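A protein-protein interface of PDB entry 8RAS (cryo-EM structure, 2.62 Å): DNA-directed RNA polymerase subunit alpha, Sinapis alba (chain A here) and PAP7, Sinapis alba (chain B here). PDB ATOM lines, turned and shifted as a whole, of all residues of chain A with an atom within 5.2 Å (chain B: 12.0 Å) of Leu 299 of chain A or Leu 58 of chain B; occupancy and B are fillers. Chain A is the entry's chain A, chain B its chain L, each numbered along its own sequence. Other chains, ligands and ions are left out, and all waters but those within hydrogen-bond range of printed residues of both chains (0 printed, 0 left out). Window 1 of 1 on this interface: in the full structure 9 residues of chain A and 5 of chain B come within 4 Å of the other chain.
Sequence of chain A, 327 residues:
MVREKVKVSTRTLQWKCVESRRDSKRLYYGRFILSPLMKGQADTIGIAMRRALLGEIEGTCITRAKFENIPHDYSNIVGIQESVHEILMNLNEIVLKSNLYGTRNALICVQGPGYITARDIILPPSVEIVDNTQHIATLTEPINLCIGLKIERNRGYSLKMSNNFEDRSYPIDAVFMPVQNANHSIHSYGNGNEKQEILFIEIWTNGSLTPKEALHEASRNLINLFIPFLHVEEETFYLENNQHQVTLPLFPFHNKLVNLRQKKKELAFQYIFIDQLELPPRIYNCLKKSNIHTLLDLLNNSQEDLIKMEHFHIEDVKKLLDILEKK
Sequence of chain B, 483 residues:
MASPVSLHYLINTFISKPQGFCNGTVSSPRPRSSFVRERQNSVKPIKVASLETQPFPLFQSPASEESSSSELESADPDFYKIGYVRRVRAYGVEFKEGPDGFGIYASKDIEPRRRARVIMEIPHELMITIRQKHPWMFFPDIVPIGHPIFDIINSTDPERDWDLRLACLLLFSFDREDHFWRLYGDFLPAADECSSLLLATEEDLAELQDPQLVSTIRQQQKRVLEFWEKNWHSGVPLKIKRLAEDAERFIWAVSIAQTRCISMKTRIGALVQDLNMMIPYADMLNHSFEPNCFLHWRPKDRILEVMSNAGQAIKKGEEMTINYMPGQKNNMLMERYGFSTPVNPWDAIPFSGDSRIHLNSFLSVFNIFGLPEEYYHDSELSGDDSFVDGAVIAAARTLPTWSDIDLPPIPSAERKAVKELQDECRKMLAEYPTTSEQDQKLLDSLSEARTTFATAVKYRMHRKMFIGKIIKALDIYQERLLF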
ATOM      1  N   PHE A 269      20.031 -17.077  -8.479  1.00  0.00           N
ATOM      2  CA  PHE A 269      19.033 -16.274  -7.780  1.00  0.00           C
ATOM      3  C   PHE A 269      18.549 -15.106  -8.629  1.00  0.00           C
ATOM      4  O   PHE A 269      17.433 -14.615  -8.424  1.00  0.00           O
ATOM      5  CB  PHE A 269      19.604 -15.764  -6.458  1.00  0.00           C
ATOM      6  CG  PHE A 269      20.013 -16.857  -5.513  1.00  0.00           C
ATOM      7  CD1 PHE A 269      19.216 -17.975  -5.341  1.00  0.00           C
ATOM      8  CD2 PHE A 269      21.198 -16.768  -4.802  1.00  0.00           C
ATOM      9  CE1 PHE A 269      19.590 -18.984  -4.474  1.00  0.00           C
ATOM     10  CE2 PHE A 269      21.578 -17.773  -3.934  1.00  0.00           C
ATOM     11  CZ  PHE A 269      20.774 -18.882  -3.770  1.00  0.00           C
ATOM     12  N   LEU A 295      15.176 -12.805  -6.778  1.00  0.00           N
ATOM     13  CA  LEU A 295      15.681 -13.313  -5.506  1.00  0.00           C
ATOM     14  C   LEU A 295      17.035 -12.704  -5.160  1.00  0.00           C
ATOM     15  O   LEU A 295      17.333 -12.475  -3.982  1.00  0.00           O
ATOM     16  CB  LEU A 295      15.773 -14.839  -5.554  1.00  0.00           C
ATOM     17  CG  LEU A 295      16.115 -15.560  -4.249  1.00  0.00           C
ATOM     18  CD1 LEU A 295      15.299 -15.003  -3.092  1.00  0.00           C
ATOM     19  CD2 LEU A 295      15.887 -17.056  -4.394  1.00  0.00           C
ATOM     20  N   LEU A 296      17.873 -12.450  -6.168  1.00  0.00           N
ATOM     21  CA  LEU A 296      19.168 -11.829  -5.910  1.00  0.00           C
ATOM     22  C   LEU A 296      19.002 -10.434  -5.324  1.00  0.00           C
ATOM     23  O   LEU A 296      19.728 -10.048  -4.400  1.00  0.00           O
ATOM     24  CB  LEU A 296      19.992 -11.778  -7.196  1.00  0.00           C
ATOM     25  CG  LEU A 296      21.389 -11.169  -7.078  1.00  0.00           C
ATOM     26  CD1 LEU A 296      22.251 -11.987  -6.131  1.00  0.00           C
ATOM     27  CD2 LEU A 296      22.043 -11.063  -8.446  1.00  0.00           C
ATOM     28  N   ASP A 297      18.047  -9.661  -5.848  1.00  0.00           N
ATOM     29  CA  ASP A 297      17.766  -8.345  -5.284  1.00  0.00           C
ATOM     30  C   ASP A 297      17.260  -8.459  -3.852  1.00  0.00           C
ATOM     31  O   ASP A 297      17.619  -7.646  -2.993  1.00  0.00           O
ATOM     32  CB  ASP A 297      16.749  -7.608  -6.154  1.00  0.00           C
ATOM     33  CG  ASP A 297      17.334  -7.151  -7.475  1.00  0.00           C
ATOM     34  OD1 ASP A 297      18.568  -6.970  -7.548  1.00  0.00           O
ATOM     35  OD2 ASP A 297      16.562  -6.975  -8.439  1.00  0.00           O
ATOM     36  N   LEU A 298      16.416  -9.458  -3.579  1.00  0.00           N
ATOM     37  CA  LEU A 298      15.914  -9.653  -2.224  1.00  0.00           C
ATOM     38  C   LEU A 298      17.047  -9.977  -1.258  1.00  0.00           C
ATOM     39  O   LEU A 298      17.092  -9.446  -0.141  1.00  0.00           O
ATOM     40  CB  LEU A 298      14.863 -10.763  -2.210  1.00  0.00           C
ATOM     41  CG  LEU A 298      14.085 -10.946  -0.907  1.00  0.00           C
ATOM     42  CD1 LEU A 298      13.568  -9.610  -0.398  1.00  0.00           C
ATOM     43  CD2 LEU A 298      12.942 -11.928  -1.101  1.00  0.00           C
ATOM     44  N   LEU A 299      17.973 -10.846  -1.670  1.00  0.00           N
ATOM     45  CA  LEU A 299      19.095 -11.194  -0.806  1.00  0.00           C
ATOM     46  C   LEU A 299      20.060 -10.028  -0.635  1.00  0.00           C
ATOM     47  O   LEU A 299      20.659  -9.874   0.435  1.00  0.00           O
ATOM     48  CB  LEU A 299      19.827 -12.414  -1.364  1.00  0.00           C
ATOM     49  CG  LEU A 299      19.013 -13.708  -1.413  1.00  0.00           C
ATOM     50  CD1 LEU A 299      19.765 -14.794  -2.164  1.00  0.00           C
ATOM     51  CD2 LEU A 299      18.657 -14.172  -0.010  1.00  0.00           C
ATOM     52  N   ASN A 300      20.226  -9.201  -1.670  1.00  0.00           N
ATOM     53  CA  ASN A 300      21.129  -8.060  -1.567  1.00  0.00           C
ATOM     54  C   ASN A 300      20.568  -6.977  -0.654  1.00  0.00           C
ATOM     55  O   ASN A 300      21.333  -6.175  -0.104  1.00  0.00           O
ATOM     56  CB  ASN A 300      21.412  -7.487  -2.955  1.00  0.00           C
ATOM     57  CG  ASN A 300      22.512  -8.234  -3.679  1.00  0.00           C
ATOM     58  OD1 ASN A 300      22.951  -9.296  -3.239  1.00  0.00           O
ATOM     59  ND2 ASN A 300      22.963  -7.683  -4.800  1.00  0.00           N
ATOM     60  N   ASN A 301      19.250  -6.932  -0.486  1.00  0.00           N
ATOM     61  CA  ASN A 301      18.633  -5.928   0.368  1.00  0.00           C
ATOM     62  C   ASN A 301      19.009  -6.153   1.829  1.00  0.00           C
ATOM     63  O   ASN A 301      19.281  -7.276   2.260  1.00  0.00           O
ATOM     64  CB  ASN A 301      17.113  -5.956   0.215  1.00  0.00           C
ATOM     65  CG  ASN A 301      16.623  -5.034  -0.880  1.00  0.00           C
ATOM     66  OD1 ASN A 301      16.071  -5.483  -1.883  1.00  0.00           O
ATOM     67  ND2 ASN A 301      16.819  -3.734  -0.692  1.00  0.00           N
ATOM     68  N   SER A 302      19.026  -5.065   2.589  1.00  0.00           N
ATOM     69  CA  SER A 302      19.298  -5.110   4.016  1.00  0.00           C
ATOM     70  C   SER A 302      18.002  -4.961   4.805  1.00  0.00           C
ATOM     71  O   SER A 302      16.996  -4.449   4.306  1.00  0.00           O
ATOM     72  CB  SER A 302      20.288  -4.012   4.418  1.00  0.00           C
ATOM     73  OG  SER A 302      19.609  -2.823   4.785  1.00  0.00           O
ATOM     74  N   GLN A 303      18.040  -5.425   6.055  1.00  0.00           N
ATOM     75  CA  GLN A 303      16.857  -5.353   6.907  1.00  0.00           C
ATOM     76  C   GLN A 303      16.480  -3.909   7.217  1.00  0.00           C
ATOM     77  O   GLN A 303      15.291  -3.577   7.296  1.00  0.00           O
ATOM     78  CB  GLN A 303      17.091  -6.138   8.198  1.00  0.00           C
ATOM     79  CG  GLN A 303      17.528  -7.576   7.974  1.00  0.00           C
ATOM     80  CD  GLN A 303      17.752  -8.327   9.271  1.00  0.00           C
ATOM     81  OE1 GLN A 303      18.484  -9.315   9.311  1.00  0.00           O
ATOM     82  NE2 GLN A 303      17.119  -7.860  10.341  1.00  0.00           N
ATOM     83  N   LEU A 306      14.453  -2.266   4.349  1.00  0.00           N
ATOM     84  CA  LEU A 306      13.082  -2.766   4.341  1.00  0.00           C
ATOM     85  C   LEU A 306      12.281  -2.216   5.513  1.00  0.00           C
ATOM     86  O   LEU A 306      11.077  -1.973   5.380  1.00  0.00           O
ATOM     87  CB  LEU A 306      13.079  -4.293   4.362  1.00  0.00           C
ATOM     88  CG  LEU A 306      13.649  -4.975   3.117  1.00  0.00           C
ATOM     89  CD1 LEU A 306      13.595  -6.487   3.258  1.00  0.00           C
ATOM     90  CD2 LEU A 306      12.908  -4.522   1.868  1.00  0.00           C
ATOM     91  N   LEU A 320       9.304 -12.950   6.843  1.00  0.00           N
ATOM     92  CA  LEU A 320       9.973 -13.041   5.550  1.00  0.00           C
ATOM     93  C   LEU A 320      11.294 -13.789   5.669  1.00  0.00           C
ATOM     94  O   LEU A 320      11.651 -14.574   4.782  1.00  0.00           O
ATOM     95  CB  LEU A 320      10.190 -11.640   4.977  1.00  0.00           C
ATOM     96  CG  LEU A 320      11.257 -11.477   3.892  1.00  0.00           C
ATOM     97  CD1 LEU A 320      10.806 -12.126   2.594  1.00  0.00           C
ATOM     98  CD2 LEU A 320      11.578 -10.005   3.678  1.00  0.00           C
ATOM     99  N   LEU A 321      12.035 -13.555   6.755  1.00  0.00           N
ATOM    100  CA  LEU A 321      13.272 -14.296   6.974  1.00  0.00           C
ATOM    101  C   LEU A 321      12.997 -15.785   7.142  1.00  0.00           C
ATOM    102  O   LEU A 321      13.740 -16.622   6.621  1.00  0.00           O
ATOM    103  CB  LEU A 321      14.011 -13.741   8.191  1.00  0.00           C
ATOM    104  CG  LEU A 321      15.109 -12.719   7.888  1.00  0.00           C
ATOM    105  CD1 LEU A 321      15.636 -12.103   9.174  1.00  0.00           C
ATOM    106  CD2 LEU A 321      16.235 -13.360   7.093  1.00  0.00           C
ATOM    107  N   LEU A 324      12.229 -17.190   3.678  1.00  0.00           N
ATOM    108  CA  LEU A 324      13.461 -17.359   2.913  1.00  0.00           C
ATOM    109  C   LEU A 324      14.275 -18.538   3.429  1.00  0.00           C
ATOM    110  O   LEU A 324      14.886 -19.271   2.643  1.00  0.00           O
ATOM    111  CB  LEU A 324      14.288 -16.074   2.956  1.00  0.00           C
ATOM    112  CG  LEU A 324      13.668 -14.849   2.279  1.00  0.00           C
ATOM    113  CD1 LEU A 324      14.718 -13.772   2.062  1.00  0.00           C
ATOM    114  CD2 LEU A 324      13.009 -15.235   0.962  1.00  0.00           C
ATOM    115  N   PHE B  56      24.941 -13.103   2.760  1.00  0.00           N
ATOM    116  CA  PHE B  56      24.044 -12.131   2.147  1.00  0.00           C
ATOM    117  C   PHE B  56      23.687 -11.025   3.135  1.00  0.00           C
ATOM    118  O   PHE B  56      23.582 -11.274   4.336  1.00  0.00           O
ATOM    119  CB  PHE B  56      22.775 -12.820   1.638  1.00  0.00           C
ATOM    120  CG  PHE B  56      22.985 -13.627   0.389  1.00  0.00           C
ATOM    121  CD1 PHE B  56      23.406 -13.018  -0.782  1.00  0.00           C
ATOM    122  CD2 PHE B  56      22.766 -14.994   0.386  1.00  0.00           C
ATOM    123  CE1 PHE B  56      23.601 -13.759  -1.932  1.00  0.00           C
ATOM    124  CE2 PHE B  56      22.960 -15.739  -0.760  1.00  0.00           C
ATOM    125  CZ  PHE B  56      23.378 -15.120  -1.921  1.00  0.00           C
ATOM    126  N   PRO B  57      23.515  -9.801   2.628  1.00  0.00           N
ATOM    127  CA  PRO B  57      23.176  -8.681   3.522  1.00  0.00           C
ATOM    128  C   PRO B  57      21.888  -8.885   4.300  1.00  0.00           C
ATOM    129  O   PRO B  57      21.797  -8.442   5.452  1.00  0.00           O
ATOM    130  CB  PRO B  57      23.070  -7.490   2.560  1.00  0.00           C
ATOM    131  CG  PRO B  57      23.918  -7.871   1.392  1.00  0.00           C
ATOM    132  CD  PRO B  57      23.755  -9.355   1.245  1.00  0.00           C
ATOM    133  N   LEU B  58      20.886  -9.538   3.708  1.00  0.00           N
ATOM    134  CA  LEU B  58      19.617  -9.725   4.407  1.00  0.00           C
ATOM    135  C   LEU B  58      19.754 -10.708   5.562  1.00  0.00           C
ATOM    136  O   LEU B  58      19.165 -10.505   6.630  1.00  0.00           O
ATOM    137  CB  LEU B  58      18.541 -10.196   3.428  1.00  0.00           C
ATOM    138  CG  LEU B  58      17.102 -10.131   3.944  1.00  0.00           C
ATOM    139  CD1 LEU B  58      16.803  -8.764   4.540  1.00  0.00           C
ATOM    140  CD2 LEU B  58      16.117 -10.462   2.838  1.00  0.00           C
ATOM    141  N   PHE B  59      20.527 -11.780   5.370  1.00  0.00           N
ATOM    142  CA  PHE B  59      20.667 -12.790   6.412  1.00  0.00           C
ATOM    143  C   PHE B  59      21.482 -12.295   7.600  1.00  0.00           C
ATOM    144  O   PHE B  59      21.386 -12.878   8.686  1.00  0.00           O
ATOM    145  CB  PHE B  59      21.298 -14.057   5.833  1.00  0.00           C
ATOM    146  CG  PHE B  59      20.295 -15.070   5.358  1.00  0.00           C
ATOM    147  CD1 PHE B  59      19.572 -15.827   6.264  1.00  0.00           C
ATOM    148  CD2 PHE B  59      20.072 -15.262   4.004  1.00  0.00           C
ATOM    149  CE1 PHE B  59      18.647 -16.759   5.831  1.00  0.00           C
ATOM    150  CE2 PHE B  59      19.149 -16.192   3.564  1.00  0.00           C
ATOM    151  CZ  PHE B  59      18.436 -16.941   4.478  1.00  0.00           C
ATOM    152  N   GLN B  60      22.274 -11.242   7.425  1.00  0.00           N
ATOM    153  CA  GLN B  60      23.060 -10.687   8.520  1.00  0.00           C
ATOM    154  C   GLN B  60      22.470  -9.365   8.999  1.00  0.00           C
ATOM    155  O   GLN B  60      21.312  -9.053   8.719  1.00  0.00           O
ATOM    156  CB  GLN B  60      24.516 -10.489   8.096  1.00  0.00           C
ATOM    157  CG  GLN B  60      25.425 -10.007   9.216  1.00  0.00           C
ATOM    158  CD  GLN B  60      26.867  -9.858   8.777  1.00  0.00           C
ATOM    159  OE1 GLN B  60      27.193 -10.039   7.604  1.00  0.00           O
ATOM    160  NE2 GLN B  60      27.742  -9.528   9.719  1.00  0.00           N
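Among the printed residues, merely in contact across the chains: Leu 299 of chain A with Pro 57 of chain B, Leu 298 of chain A with Leu 58 of chain B, Asn 300 of chain A with Pro 57 of chain B, Leu 299 of chain A with Phe 56 of chain B, Leu 324 of chain A with Leu 58 of chain B, Asn 301 of chain A with Pro 57 of chain B, Phe 269 of chain A with Phe 56 of chain B and Ser 302 of chain A with Leu 58 of chain B.
O of Phe 269 of chain A sits close to N of Leu 295 of chain A, at 3.3 Å. The backbone carbonyl oxygen (O) of Phe 269 of chain A lies within hydrogen-bond range of the backbone NH (N) of Leu 296 of chain A, at 3.2 Å. The backbone carbonyl oxygen of Asp 297 of chain A sits close to the side-chain amide oxygen of Asn 301 of chain A, at 2.9 Å.
Of the 5 printed residues of chain B, 4 touch a printed residue of chain A. Hydrophobic or aromatic side chains of chain B within 4 Å of the printed part of chain A: Phe 56, Pro 57 and Leu 58. Printed residues of chain A that touch a printed residue of chain B: Phe 269, Leu 298, Leu 299, Asn 300, Asn 301, Ser 302, Gln 303 and Leu 324. Hydrophobic or aromatic side chains of chain A that line the printed part of chain B: Phe 269, Leu 299 and Leu 324. Among the printed residues, no Asp or Glu carboxylate lies within 4 Å of a Lys or Arg side-chain nitrogen of the other chain.
Leu 299 of chain A touches three residues of chain B. Of the printed residues of chain A, Leu 58 of chain B touches Leu 298 (3.3 Å), Leu 299 (3.3 Å), Asn 301 (3.1 Å), Ser 302 (3.996 Å), Gln 303 (3.0 Å) and Leu 324 (3.7 Å). Of chain B, only Phe 56 (3.8 Å) comes within 4 Å of Phe 269 of chain A. No residue of chain B comes within 4 Å of Leu 296 of chain A. No residue of chain B comes within 4 Å of Asp 297 of chain A. Leu 298 of chain A touches just one residue of chain B: Leu 58. Asn 300 of chain A touches just one residue of chain B: Pro 57 (3.4 Å). Of chain B, only Pro 57 (3.7 Å) and Leu 58 (3.1 Å) come within 4 Å of Asn 301 of chain A. Of chain B, only Leu 58 and Gln 60 come within 4 Å of Gln 303 of chain A. Of chain B, only Leu 58 (3.7 Å) comes within 4 Å of Leu 324 of chain A. Of the printed residues of chain B, Ser 302 of chain A touches Leu 58. Of the printed residues of chain A, Pro 57 of chain B touches Leu 299 (3.2 Å), Asn 300 (3.4 Å) and Asn 301 (3.7 Å). Printed residues of chain A within 4 Å of Gln 60 of chain B: Gln 303. Of the printed residues of chain A, Phe 56 of chain B touches Phe 269 (3.8 Å) and Leu 299 (3.6 Å). Phe 59 of chain B touches none of the printed residues of chain A. The nearest residue of chain B that does not touch Leu 299 of chain A is Phe 59 of chain B (4.1 Å).
The backbone NH of Leu 58 of chain B lies within hydrogen-bond range of the backbone carbonyl oxygen of Leu 299 of chain A (3.3 Å). The backbone NH (N) of Leu 58 of chain B lies within hydrogen-bond range of the backbone carbonyl oxygen (O) of Asn 301 of chain A, 3.1 Å away. The backbone carbonyl oxygen (O) of Leu 58 of chain B sits close to the side-chain amide oxygen (OE1) of Gln 303 of chain A (3.0 Å). O of Gln 60 of chain B lies close to OE1 of Gln 303 of chain A (2.9 Å).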
